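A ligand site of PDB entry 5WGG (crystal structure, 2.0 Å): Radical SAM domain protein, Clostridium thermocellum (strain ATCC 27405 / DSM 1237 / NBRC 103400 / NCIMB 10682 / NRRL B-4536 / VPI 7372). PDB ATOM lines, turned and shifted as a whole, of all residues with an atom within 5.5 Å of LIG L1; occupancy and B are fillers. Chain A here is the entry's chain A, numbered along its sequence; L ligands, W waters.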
ATOM      1  N   CYS A 107       2.812  18.840   3.912  1.00  0.00           N
ATOM      2  CA  CYS A 107       2.243  18.437   5.183  1.00  0.00           C
ATOM      3  C   CYS A 107       3.118  17.337   5.759  1.00  0.00           C
ATOM      4  O   CYS A 107       3.982  16.792   5.070  1.00  0.00           O
ATOM      5  CB  CYS A 107       0.803  18.000   5.053  1.00  0.00           C
ATOM      6  SG  CYS A 107       0.307  17.358   6.612  1.00  0.00           S
ATOM      7  N   TYR A 113      -8.264  10.432   2.695  1.00  0.00           N
ATOM      8  CA  TYR A 113      -9.381  11.121   2.033  1.00  0.00           C
ATOM      9  C   TYR A 113      -9.033  12.539   1.550  1.00  0.00           C
ATOM     10  O   TYR A 113      -9.880  13.201   0.951  1.00  0.00           O
ATOM     11  CB  TYR A 113     -10.630  11.184   2.957  1.00  0.00           C
ATOM     12  CG  TYR A 113     -10.346  11.605   4.386  1.00  0.00           C
ATOM     13  CD1 TYR A 113      -9.800  12.847   4.658  1.00  0.00           C
ATOM     14  CD2 TYR A 113     -10.616  10.745   5.467  1.00  0.00           C
ATOM     15  CE1 TYR A 113      -9.506  13.238   5.955  1.00  0.00           C
ATOM     16  CE2 TYR A 113     -10.325  11.131   6.783  1.00  0.00           C
ATOM     17  CZ  TYR A 113      -9.767  12.393   7.010  1.00  0.00           C
ATOM     18  OH  TYR A 113      -9.441  12.856   8.258  1.00  0.00           O
ATOM     19  N   CYS A 114      -7.825  13.019   1.786  1.00  0.00           N
ATOM     20  CA  CYS A 114      -7.524  14.434   1.619  1.00  0.00           C
ATOM     21  C   CYS A 114      -7.048  14.785   0.202  1.00  0.00           C
ATOM     22  O   CYS A 114      -6.372  13.991  -0.469  1.00  0.00           O
ATOM     23  CB  CYS A 114      -6.460  14.847   2.630  1.00  0.00           C
ATOM     24  SG  CYS A 114      -6.117  16.559   2.474  1.00  0.00           S
ATOM     25  N   PHE A 115      -7.358  16.018  -0.216  1.00  0.00           N
ATOM     26  CA  PHE A 115      -6.874  16.513  -1.511  1.00  0.00           C
ATOM     27  C   PHE A 115      -5.359  16.649  -1.529  1.00  0.00           C
ATOM     28  O   PHE A 115      -4.745  16.595  -2.597  1.00  0.00           O
ATOM     29  CB  PHE A 115      -7.522  17.867  -1.843  1.00  0.00           C
ATOM     30  CG  PHE A 115      -7.014  19.014  -1.015  1.00  0.00           C
ATOM     31  CD1 PHE A 115      -7.562  19.275   0.243  1.00  0.00           C
ATOM     32  CD2 PHE A 115      -5.992  19.835  -1.479  1.00  0.00           C
ATOM     33  CE1 PHE A 115      -7.084  20.325   1.020  1.00  0.00           C
ATOM     34  CE2 PHE A 115      -5.523  20.891  -0.703  1.00  0.00           C
ATOM     35  CZ  PHE A 115      -6.072  21.130   0.550  1.00  0.00           C
ATOM     36  N   PHE A 155      -4.767  27.738   6.278  1.00  0.00           N
ATOM     37  CA  PHE A 155      -5.162  26.426   5.805  1.00  0.00           C
ATOM     38  C   PHE A 155      -4.005  25.825   5.019  1.00  0.00           C
ATOM     39  O   PHE A 155      -2.863  26.302   5.095  1.00  0.00           O
ATOM     40  CB  PHE A 155      -6.385  26.570   4.889  1.00  0.00           C
ATOM     41  CG  PHE A 155      -7.300  25.356   4.809  1.00  0.00           C
ATOM     42  CD1 PHE A 155      -8.153  25.030   5.872  1.00  0.00           C
ATOM     43  CD2 PHE A 155      -7.402  24.622   3.637  1.00  0.00           C
ATOM     44  CE1 PHE A 155      -9.046  23.956   5.769  1.00  0.00           C
ATOM     45  CE2 PHE A 155      -8.299  23.540   3.531  1.00  0.00           C
ATOM     46  CZ  PHE A 155      -9.125  23.221   4.600  1.00  0.00           C
ATOM     47  N   GLY A 156      -4.304  24.807   4.241  1.00  0.00           N
ATOM     48  CA  GLY A 156      -3.410  24.416   3.178  1.00  0.00           C
ATOM     49  C   GLY A 156      -3.334  22.931   3.258  1.00  0.00           C
ATOM     50  O   GLY A 156      -4.354  22.248   3.266  1.00  0.00           O
ATOM     51  N   GLY A 157      -2.098  22.454   3.242  1.00  0.00           N
ATOM     52  CA  GLY A 157      -1.717  21.259   3.945  1.00  0.00           C
ATOM     53  C   GLY A 157      -1.624  21.709   5.388  1.00  0.00           C
ATOM     54  O   GLY A 157      -2.618  22.198   5.934  1.00  0.00           O
ATOM     55  N   GLU A 158      -0.431  21.597   5.993  1.00  0.00           N
ATOM     56  CA  GLU A 158      -0.339  21.982   7.388  1.00  0.00           C
ATOM     57  C   GLU A 158       0.186  23.403   7.524  1.00  0.00           C
ATOM     58  O   GLU A 158       1.387  23.640   7.277  1.00  0.00           O
ATOM     59  CB  GLU A 158       0.549  21.017   8.168  1.00  0.00           C
ATOM     60  CG  GLU A 158       0.774  21.554   9.532  1.00  0.00           C
ATOM     61  CD  GLU A 158      -0.555  21.705  10.234  1.00  0.00           C
ATOM     62  OE1 GLU A 158      -1.475  20.898   9.965  1.00  0.00           O
ATOM     63  OE2 GLU A 158      -0.683  22.641  11.030  1.00  0.00           O
ATOM     64  N   PRO A 159      -0.655  24.376   7.919  1.00  0.00           N
ATOM     65  CA  PRO A 159      -0.191  25.787   7.979  1.00  0.00           C
ATOM     66  C   PRO A 159       0.943  26.018   8.955  1.00  0.00           C
ATOM     67  O   PRO A 159       1.806  26.876   8.703  1.00  0.00           O
ATOM     68  CB  PRO A 159      -1.456  26.543   8.430  1.00  0.00           C
ATOM     69  CG  PRO A 159      -2.404  25.471   8.978  1.00  0.00           C
ATOM     70  CD  PRO A 159      -2.090  24.237   8.223  1.00  0.00           C
ATOM     71  N   THR A 189      -6.561  26.027  11.060  1.00  0.00           N
ATOM     72  CA  THR A 189      -6.947  24.616  11.045  1.00  0.00           C
ATOM     73  C   THR A 189      -5.664  23.814  10.994  1.00  0.00           C
ATOM     74  O   THR A 189      -4.862  23.998  10.075  1.00  0.00           O
ATOM     75  CB  THR A 189      -7.835  24.298   9.828  1.00  0.00           C
ATOM     76  OG1 THR A 189      -8.906  25.244   9.755  1.00  0.00           O
ATOM     77  CG2 THR A 189      -8.435  22.922   9.952  1.00  0.00           C
ATOM     78  N   THR A 190      -5.426  22.973  12.004  1.00  0.00           N
ATOM     79  CA  THR A 190      -4.151  22.264  12.071  1.00  0.00           C
ATOM     80  C   THR A 190      -4.370  20.804  12.440  1.00  0.00           C
ATOM     81  O   THR A 190      -5.307  20.452  13.166  1.00  0.00           O
ATOM     82  CB  THR A 190      -3.181  22.917  13.063  1.00  0.00           C
ATOM     83  OG1 THR A 190      -1.985  22.130  13.138  1.00  0.00           O
ATOM     84  CG2 THR A 190      -3.816  22.993  14.469  1.00  0.00           C
ATOM     85  N   ASN A 191      -3.476  19.957  11.910  1.00  0.00           N
ATOM     86  CA  ASN A 191      -3.421  18.556  12.291  1.00  0.00           C
ATOM     87  C   ASN A 191      -2.823  18.351  13.677  1.00  0.00           C
ATOM     88  O   ASN A 191      -2.840  17.214  14.166  1.00  0.00           O
ATOM     89  CB  ASN A 191      -2.644  17.715  11.259  1.00  0.00           C
ATOM     90  CG  ASN A 191      -1.118  18.011  11.211  1.00  0.00           C
ATOM     91  OD1 ASN A 191      -0.521  18.608  12.102  1.00  0.00           O
ATOM     92  ND2 ASN A 191      -0.499  17.579  10.120  1.00  0.00           N
ATOM     93  N   VAL A 211      -9.366  25.157  14.556  1.00  0.00           N
ATOM     94  CA  VAL A 211     -10.013  23.895  14.229  1.00  0.00           C
ATOM     95  C   VAL A 211      -8.976  22.793  14.392  1.00  0.00           C
ATOM     96  O   VAL A 211      -7.872  22.883  13.838  1.00  0.00           O
ATOM     97  CB  VAL A 211     -10.602  23.931  12.801  1.00  0.00           C
ATOM     98  CG1 VAL A 211     -11.127  22.577  12.409  1.00  0.00           C
ATOM     99  CG2 VAL A 211     -11.725  24.989  12.726  1.00  0.00           C
ATOM    100  N   LEU A 212      -9.329  21.769  15.154  1.00  0.00           N
ATOM    101  CA  LEU A 212      -8.376  20.712  15.492  1.00  0.00           C
ATOM    102  C   LEU A 212      -8.847  19.399  14.900  1.00  0.00           C
ATOM    103  O   LEU A 212      -9.922  18.904  15.240  1.00  0.00           O
ATOM    104  CB  LEU A 212      -8.196  20.630  17.013  1.00  0.00           C
ATOM    105  CG  LEU A 212      -8.008  21.958  17.768  1.00  0.00           C
ATOM    106  CD1 LEU A 212      -8.224  21.828  19.299  1.00  0.00           C
ATOM    107  CD2 LEU A 212      -6.586  22.483  17.509  1.00  0.00           C
ATOM    108  N   SER A 213      -8.024  18.812  14.026  1.00  0.00           N
ATOM    109  CA  SER A 213      -8.469  17.676  13.202  1.00  0.00           C
ATOM    110  C   SER A 213      -8.172  16.354  13.888  1.00  0.00           C
ATOM    111  O   SER A 213      -7.004  16.012  14.104  1.00  0.00           O
ATOM    112  CB  SER A 213      -7.806  17.712  11.841  1.00  0.00           C
ATOM    113  OG  SER A 213      -8.119  18.928  11.208  1.00  0.00           O
ATOM    114  N   ASP A 215     -10.377  12.332  14.046  1.00  0.00           N
ATOM    115  CA  ASP A 215     -11.554  11.683  13.467  1.00  0.00           C
ATOM    116  C   ASP A 215     -12.361  10.867  14.485  1.00  0.00           C
ATOM    117  O   ASP A 215     -13.430  10.362  14.141  1.00  0.00           O
ATOM    118  CB  ASP A 215     -11.136  10.810  12.279  1.00  0.00           C
ATOM    119  CG  ASP A 215     -10.765  11.657  11.044  1.00  0.00           C
ATOM    120  OD1 ASP A 215     -11.142  12.857  11.025  1.00  0.00           O
ATOM    121  OD2 ASP A 215     -10.131  11.118  10.096  1.00  0.00           O
ATOM    122  N   ARG A 225      -5.563   9.001   9.194  1.00  0.00           N
ATOM    123  CA  ARG A 225      -4.657  10.140   9.326  1.00  0.00           C
ATOM    124  C   ARG A 225      -3.264   9.615   9.671  1.00  0.00           C
ATOM    125  O   ARG A 225      -2.963   9.341  10.839  1.00  0.00           O
ATOM    126  CB  ARG A 225      -5.201  11.146  10.338  1.00  0.00           C
ATOM    127  CG  ARG A 225      -6.633  11.582  10.005  1.00  0.00           C
ATOM    128  CD  ARG A 225      -7.181  12.658  10.961  1.00  0.00           C
ATOM    129  NE  ARG A 225      -6.334  13.851  11.002  1.00  0.00           N
ATOM    130  CZ  ARG A 225      -6.331  14.816  10.078  1.00  0.00           C
ATOM    131  NH1 ARG A 225      -5.511  15.844  10.219  1.00  0.00           N
ATOM    132  NH2 ARG A 225      -7.152  14.787   9.022  1.00  0.00           N
ATOM    133  N   ARG A 256     -12.525  18.582  14.721  1.00  0.00           N
ATOM    134  CA  ARG A 256     -13.182  18.364  13.435  1.00  0.00           C
ATOM    135  C   ARG A 256     -12.825  16.975  12.910  1.00  0.00           C
ATOM    136  O   ARG A 256     -11.661  16.697  12.585  1.00  0.00           O
ATOM    137  CB  ARG A 256     -12.770  19.459  12.450  1.00  0.00           C
ATOM    138  CG  ARG A 256     -13.025  19.165  10.955  1.00  0.00           C
ATOM    139  CD  ARG A 256     -14.478  19.196  10.545  1.00  0.00           C
ATOM    140  NE  ARG A 256     -14.555  19.545   9.122  1.00  0.00           N
ATOM    141  CZ  ARG A 256     -14.297  18.705   8.123  1.00  0.00           C
ATOM    142  NH1 ARG A 256     -13.976  17.441   8.378  1.00  0.00           N
ATOM    143  NH2 ARG A 256     -14.356  19.116   6.867  1.00  0.00           N
ATOM    144  N   THR A 258     -13.766  13.674  10.136  1.00  0.00           N
ATOM    145  CA  THR A 258     -14.333  13.328   8.833  1.00  0.00           C
ATOM    146  C   THR A 258     -14.694  11.865   8.894  1.00  0.00           C
ATOM    147  O   THR A 258     -13.835  11.046   9.213  1.00  0.00           O
ATOM    148  CB  THR A 258     -13.317  13.575   7.706  1.00  0.00           C
ATOM    149  OG1 THR A 258     -12.841  14.925   7.753  1.00  0.00           O
ATOM    150  CG2 THR A 258     -13.928  13.228   6.312  1.00  0.00           C
ATOM    151  N   PRO A 285     -19.477  14.165   6.910  1.00  0.00           N
ATOM    152  CA  PRO A 285     -19.196  13.179   5.846  1.00  0.00           C
ATOM    153  C   PRO A 285     -18.084  13.645   4.898  1.00  0.00           C
ATOM    154  O   PRO A 285     -17.944  14.828   4.589  1.00  0.00           O
ATOM    155  CB  PRO A 285     -20.534  13.029   5.127  1.00  0.00           C
ATOM    156  CG  PRO A 285     -21.304  14.284   5.429  1.00  0.00           C
ATOM    157  CD  PRO A 285     -20.823  14.766   6.782  1.00  0.00           C
ATOM    158  N   VAL A 286     -17.299  12.670   4.430  1.00  0.00           N
ATOM    159  CA  VAL A 286     -16.219  12.917   3.472  1.00  0.00           C
ATOM    160  C   VAL A 286     -16.758  13.597   2.209  1.00  0.00           C
ATOM    161  O   VAL A 286     -17.833  13.254   1.686  1.00  0.00           O
ATOM    162  CB  VAL A 286     -15.503  11.604   3.114  1.00  0.00           C
ATOM    163  CG1 VAL A 286     -16.490  10.617   2.482  1.00  0.00           C
ATOM    164  CG2 VAL A 286     -14.332  11.851   2.182  1.00  0.00           C
ATOM    165  N   VAL A 287     -15.978  14.558   1.696  1.00  0.00           N
ATOM    166  CA  VAL A 287     -16.303  15.314   0.491  1.00  0.00           C
ATOM    167  C   VAL A 287     -15.509  14.759  -0.695  1.00  0.00           C
ATOM    168  O   VAL A 287     -14.322  14.407  -0.552  1.00  0.00           O
ATOM    169  CB  VAL A 287     -15.992  16.807   0.692  1.00  0.00           C
ATOM    170  CG1 VAL A 287     -16.089  17.573  -0.627  1.00  0.00           C
ATOM    171  CG2 VAL A 287     -16.911  17.421   1.808  1.00  0.00           C
ATOM    172  N   ALA A 288     -16.151  14.695  -1.864  1.00  0.00           N
ATOM    173  CA  ALA A 288     -15.488  14.430  -3.156  1.00  0.00           C
ATOM    174  C   ALA A 288     -14.740  13.093  -3.158  1.00  0.00           C
ATOM    175  O   ALA A 288     -13.598  12.991  -3.608  1.00  0.00           O
ATOM    176  CB  ALA A 288     -14.565  15.589  -3.540  1.00  0.00           C
ATOM    177  N   HIS A 366     -10.824  25.000  -1.545  1.00  0.00           N
ATOM    178  CA  HIS A 366      -9.712  24.064  -1.494  1.00  0.00           C
ATOM    179  C   HIS A 366      -9.993  22.792  -2.292  1.00  0.00           C
ATOM    180  O   HIS A 366      -9.044  22.167  -2.755  1.00  0.00           O
ATOM    181  CB  HIS A 366      -9.380  23.720  -0.045  1.00  0.00           C
ATOM    182  CG  HIS A 366     -10.319  22.727   0.568  1.00  0.00           C
ATOM    183  ND1 HIS A 366      -9.965  21.418   0.796  1.00  0.00           N
ATOM    184  CD2 HIS A 366     -11.597  22.850   0.968  1.00  0.00           C
ATOM    185  CE1 HIS A 366     -10.981  20.773   1.328  1.00  0.00           C
ATOM    186  NE2 HIS A 366     -12.000  21.619   1.447  1.00  0.00           N
ATOM    187  N   GLN A 367     -11.250  22.410  -2.491  1.00  0.00           N
ATOM    188  CA  GLN A 367     -11.470  21.167  -3.229  1.00  0.00           C
ATOM    189  C   GLN A 367     -11.290  21.317  -4.731  1.00  0.00           C
ATOM    190  O   GLN A 367     -11.195  20.307  -5.436  1.00  0.00           O
ATOM    191  CB  GLN A 367     -12.870  20.623  -2.919  1.00  0.00           C
ATOM    192  CG  GLN A 367     -13.061  20.106  -1.483  1.00  0.00           C
ATOM    193  CD  GLN A 367     -12.431  18.734  -1.274  1.00  0.00           C
ATOM    194  OE1 GLN A 367     -12.182  18.002  -2.226  1.00  0.00           O
ATOM    195  NE2 GLN A 367     -12.171  18.372  -0.031  1.00  0.00           N
HETATM  196  N1  LIG L   1      -3.580  20.578   7.931  1.00  0.00           N
HETATM  197  C1  LIG L   1      -4.750  21.186   8.550  1.00  0.00           C
HETATM  198  C2  LIG L   1      -5.638  20.149   9.275  1.00  0.00           C
HETATM  199  O1  LIG L   1      -5.626  18.939   9.017  1.00  0.00           O
HETATM  200  O2  LIG L   1      -6.402  20.517  10.166  1.00  0.00           O
HETATM  201  C3  LIG L   1      -5.546  21.995   7.526  1.00  0.00           C
HETATM  202  C4  LIG L   1      -5.783  21.298   6.192  1.00  0.00           C
HETATM  203  S1  LIG L   1      -6.899  19.881   6.254  1.00  0.00           S
HETATM  204  C5  LIG L   1      -7.602  19.780   4.581  1.00  0.00           C
HETATM  205  C6  LIG L   1      -8.334  20.645   7.116  1.00  0.00           C
HETATM  206  C7  LIG L   1      -9.549  19.760   7.456  1.00  0.00           C
HETATM  207  O3  LIG L   1     -10.211  19.275   6.289  1.00  0.00           O
HETATM  208  C8  LIG L   1      -9.137  18.524   8.258  1.00  0.00           C
HETATM  209  O4  LIG L   1      -9.977  18.345   9.393  1.00  0.00           O
HETATM  210  C9  LIG L   1      -9.383  17.386   7.301  1.00  0.00           C
HETATM  211  O5  LIG L   1      -9.770  16.237   7.994  1.00  0.00           O
HETATM  212  C10 LIG L   1     -10.536  17.921   6.457  1.00  0.00           C
HETATM  213  N2  LIG L   1     -10.629  17.195   5.183  1.00  0.00           N
HETATM  214  C11 LIG L   1      -9.576  16.856   4.362  1.00  0.00           C
HETATM  215  N3  LIG L   1     -10.078  16.191   3.282  1.00  0.00           N
HETATM  216  C12 LIG L   1     -11.422  16.098   3.384  1.00  0.00           C
HETATM  217  C13 LIG L   1     -12.421  15.528   2.575  1.00  0.00           C
HETATM  218  N4  LIG L   1     -12.156  14.896   1.452  1.00  0.00           N
HETATM  219  N5  LIG L   1     -13.737  15.581   2.960  1.00  0.00           N
HETATM  220  C14 LIG L   1     -14.053  16.207   4.145  1.00  0.00           C
HETATM  221  N6  LIG L   1     -13.071  16.768   4.938  1.00  0.00           N
HETATM  222  C15 LIG L   1     -11.779  16.715   4.590  1.00  0.00           C
HETATM  223 FE1  LG2 L   2      -4.452  18.456   6.975  1.00  0.00          FE
HETATM  224 FE2  LG2 L   2      -2.037  17.362   5.584  1.00  0.00          FE
HETATM  225 FE3  LG2 L   2      -4.676  16.941   4.425  1.00  0.00          FE
HETATM  226 FE4  LG2 L   2      -3.951  15.409   6.675  1.00  0.00          FE
HETATM  227  S1  LG2 L   2      -2.968  15.570   4.733  1.00  0.00           S
HETATM  228  S2  LG2 L   2      -5.663  16.752   6.348  1.00  0.00           S
HETATM  229  S3  LG2 L   2      -2.867  17.050   7.608  1.00  0.00           S
HETATM  230  S4  LG2 L   2      -3.641  18.775   4.928  1.00  0.00           S
HETATM  231  O   HOH W   1     -10.584  15.834  10.416  1.00  0.00           O
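The side-chain hydroxyl (OG) of Ser 213 is in hydrogen-bond range of an oxygen (O2) of LIG L1, 2.6 Å away. O of Gly 157 sits close to N1 of LIG L1, 2.7 Å away. The backbone NH (N) of Val 287 is in hydrogen-bond range of a nitrogen (N5) of LIG L1 (2.8 Å). A nitrogen (N4) of LIG L1 is in hydrogen-bond range of the backbone carbonyl oxygen of Val 287, at 3.0 Å. The backbone carbonyl oxygen (O) of Tyr 113 lies within hydrogen-bond range of a nitrogen (N4) of LIG L1 (2.9 Å). OH of Tyr 113 lies within hydrogen-bond range of O5 of LIG L1 (3.4 Å). OE1 of Glu 158 lies close to N1 of LIG L1. The backbone NH of Thr 190 sits close to an oxygen (O2) of LIG L1 (3.2 Å). NH2 of Arg 225 is in hydrogen-bond range of O5 of LIG L1, 3.2 Å away. The guanidinium group (NH2) of Arg 256 sits at hydrogen-bond distance from a nitrogen (N6) of LIG L1 (3.3 Å). An oxygen (O5) of LIG L1 lies within hydrogen-bond range of the side-chain hydroxyl (OG1) of Thr 258 (3.3 Å). O2 of LIG L1 sits close to N of Asn 191. A sulfur (S2) of LG2 L2 sits close to the guanidinium group (NH2) of Arg 225, 3.6 Å away. The side-chain amide nitrogen (ND2) of Asn 191 lies close to a sulfur (S3) of LG2 L2 (3.5 Å). SG of Cys 114 is bound to FE3 of LG2 L2. An iron atom (FE2) of LG2 L2 is bound by the side-chain sulfur of Cys 107, at 2.6 Å.
An oxygen (O1) of LIG L1 binds an iron atom (FE1) of LG2 L2.
The backbone carbonyl oxygen of Thr 190 lies within hydrogen-bond range of the backbone NH of Ser 213 (3.3 Å). The side-chain hydroxyl (OH) of Tyr 113 is in hydrogen-bond range of the guanidinium group (NH2) of Arg 225 (3.1 Å). The side-chain hydroxyl (OH) of Tyr 113 sits at hydrogen-bond distance from the side-chain carboxylate (OD2) of Asp 215 (2.6 Å). OE2 of Glu 158 lies within hydrogen-bond range of OG1 of Thr 190 (2.5 Å). The guanidinium group (NH1) of Arg 256 lies within hydrogen-bond range of the side-chain hydroxyl (OG1) of Thr 258, at 2.8 Å. N of Arg 256 lies within hydrogen-bond range of O of Leu 212, 2.7 Å away. The side-chain carboxylate (OD1) of Asp 215 sits at hydrogen-bond distance from the backbone NH (N) of Thr 258 (2.9 Å). ND2 of Asn 191 lies close to SG of Cys 107.
Cys 114 touches LIG L1 (CA to N3, 3.5 Å). Phe 115 touches LIG L1. Phe 155 touches LIG L1 (CE1 to C6, 3.6 Å). O of Gly 156 touches C4 of LIG L1 (3.4 Å). CD of Pro 159 touches N1 of LIG L1, at 3.96 Å. Thr 189 touches LIG L1 (CG2 to O2, 3.2 Å). CA of Val 286 touches N5 of LIG L1, 3.7 Å away. NE2 of Gln 367 touches N4 of LIG L1, 3.8 Å away. 18 residues have an atom within 4 Å of LIG L1: Tyr 113, Cys 114, Phe 115, Phe 155, Gly 156, Gly 157, Glu 158, Pro 159, Thr 189, Thr 190, Asn 191, Ser 213, Arg 225, Arg 256, Thr 258, Val 286, Val 287 and Gln 367.
Water W1 lies within hydrogen-bond range of the backbone carbonyl oxygen of Arg 256, an oxygen (O5) of LIG L1 and the side-chain carboxylate of Asp 215.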
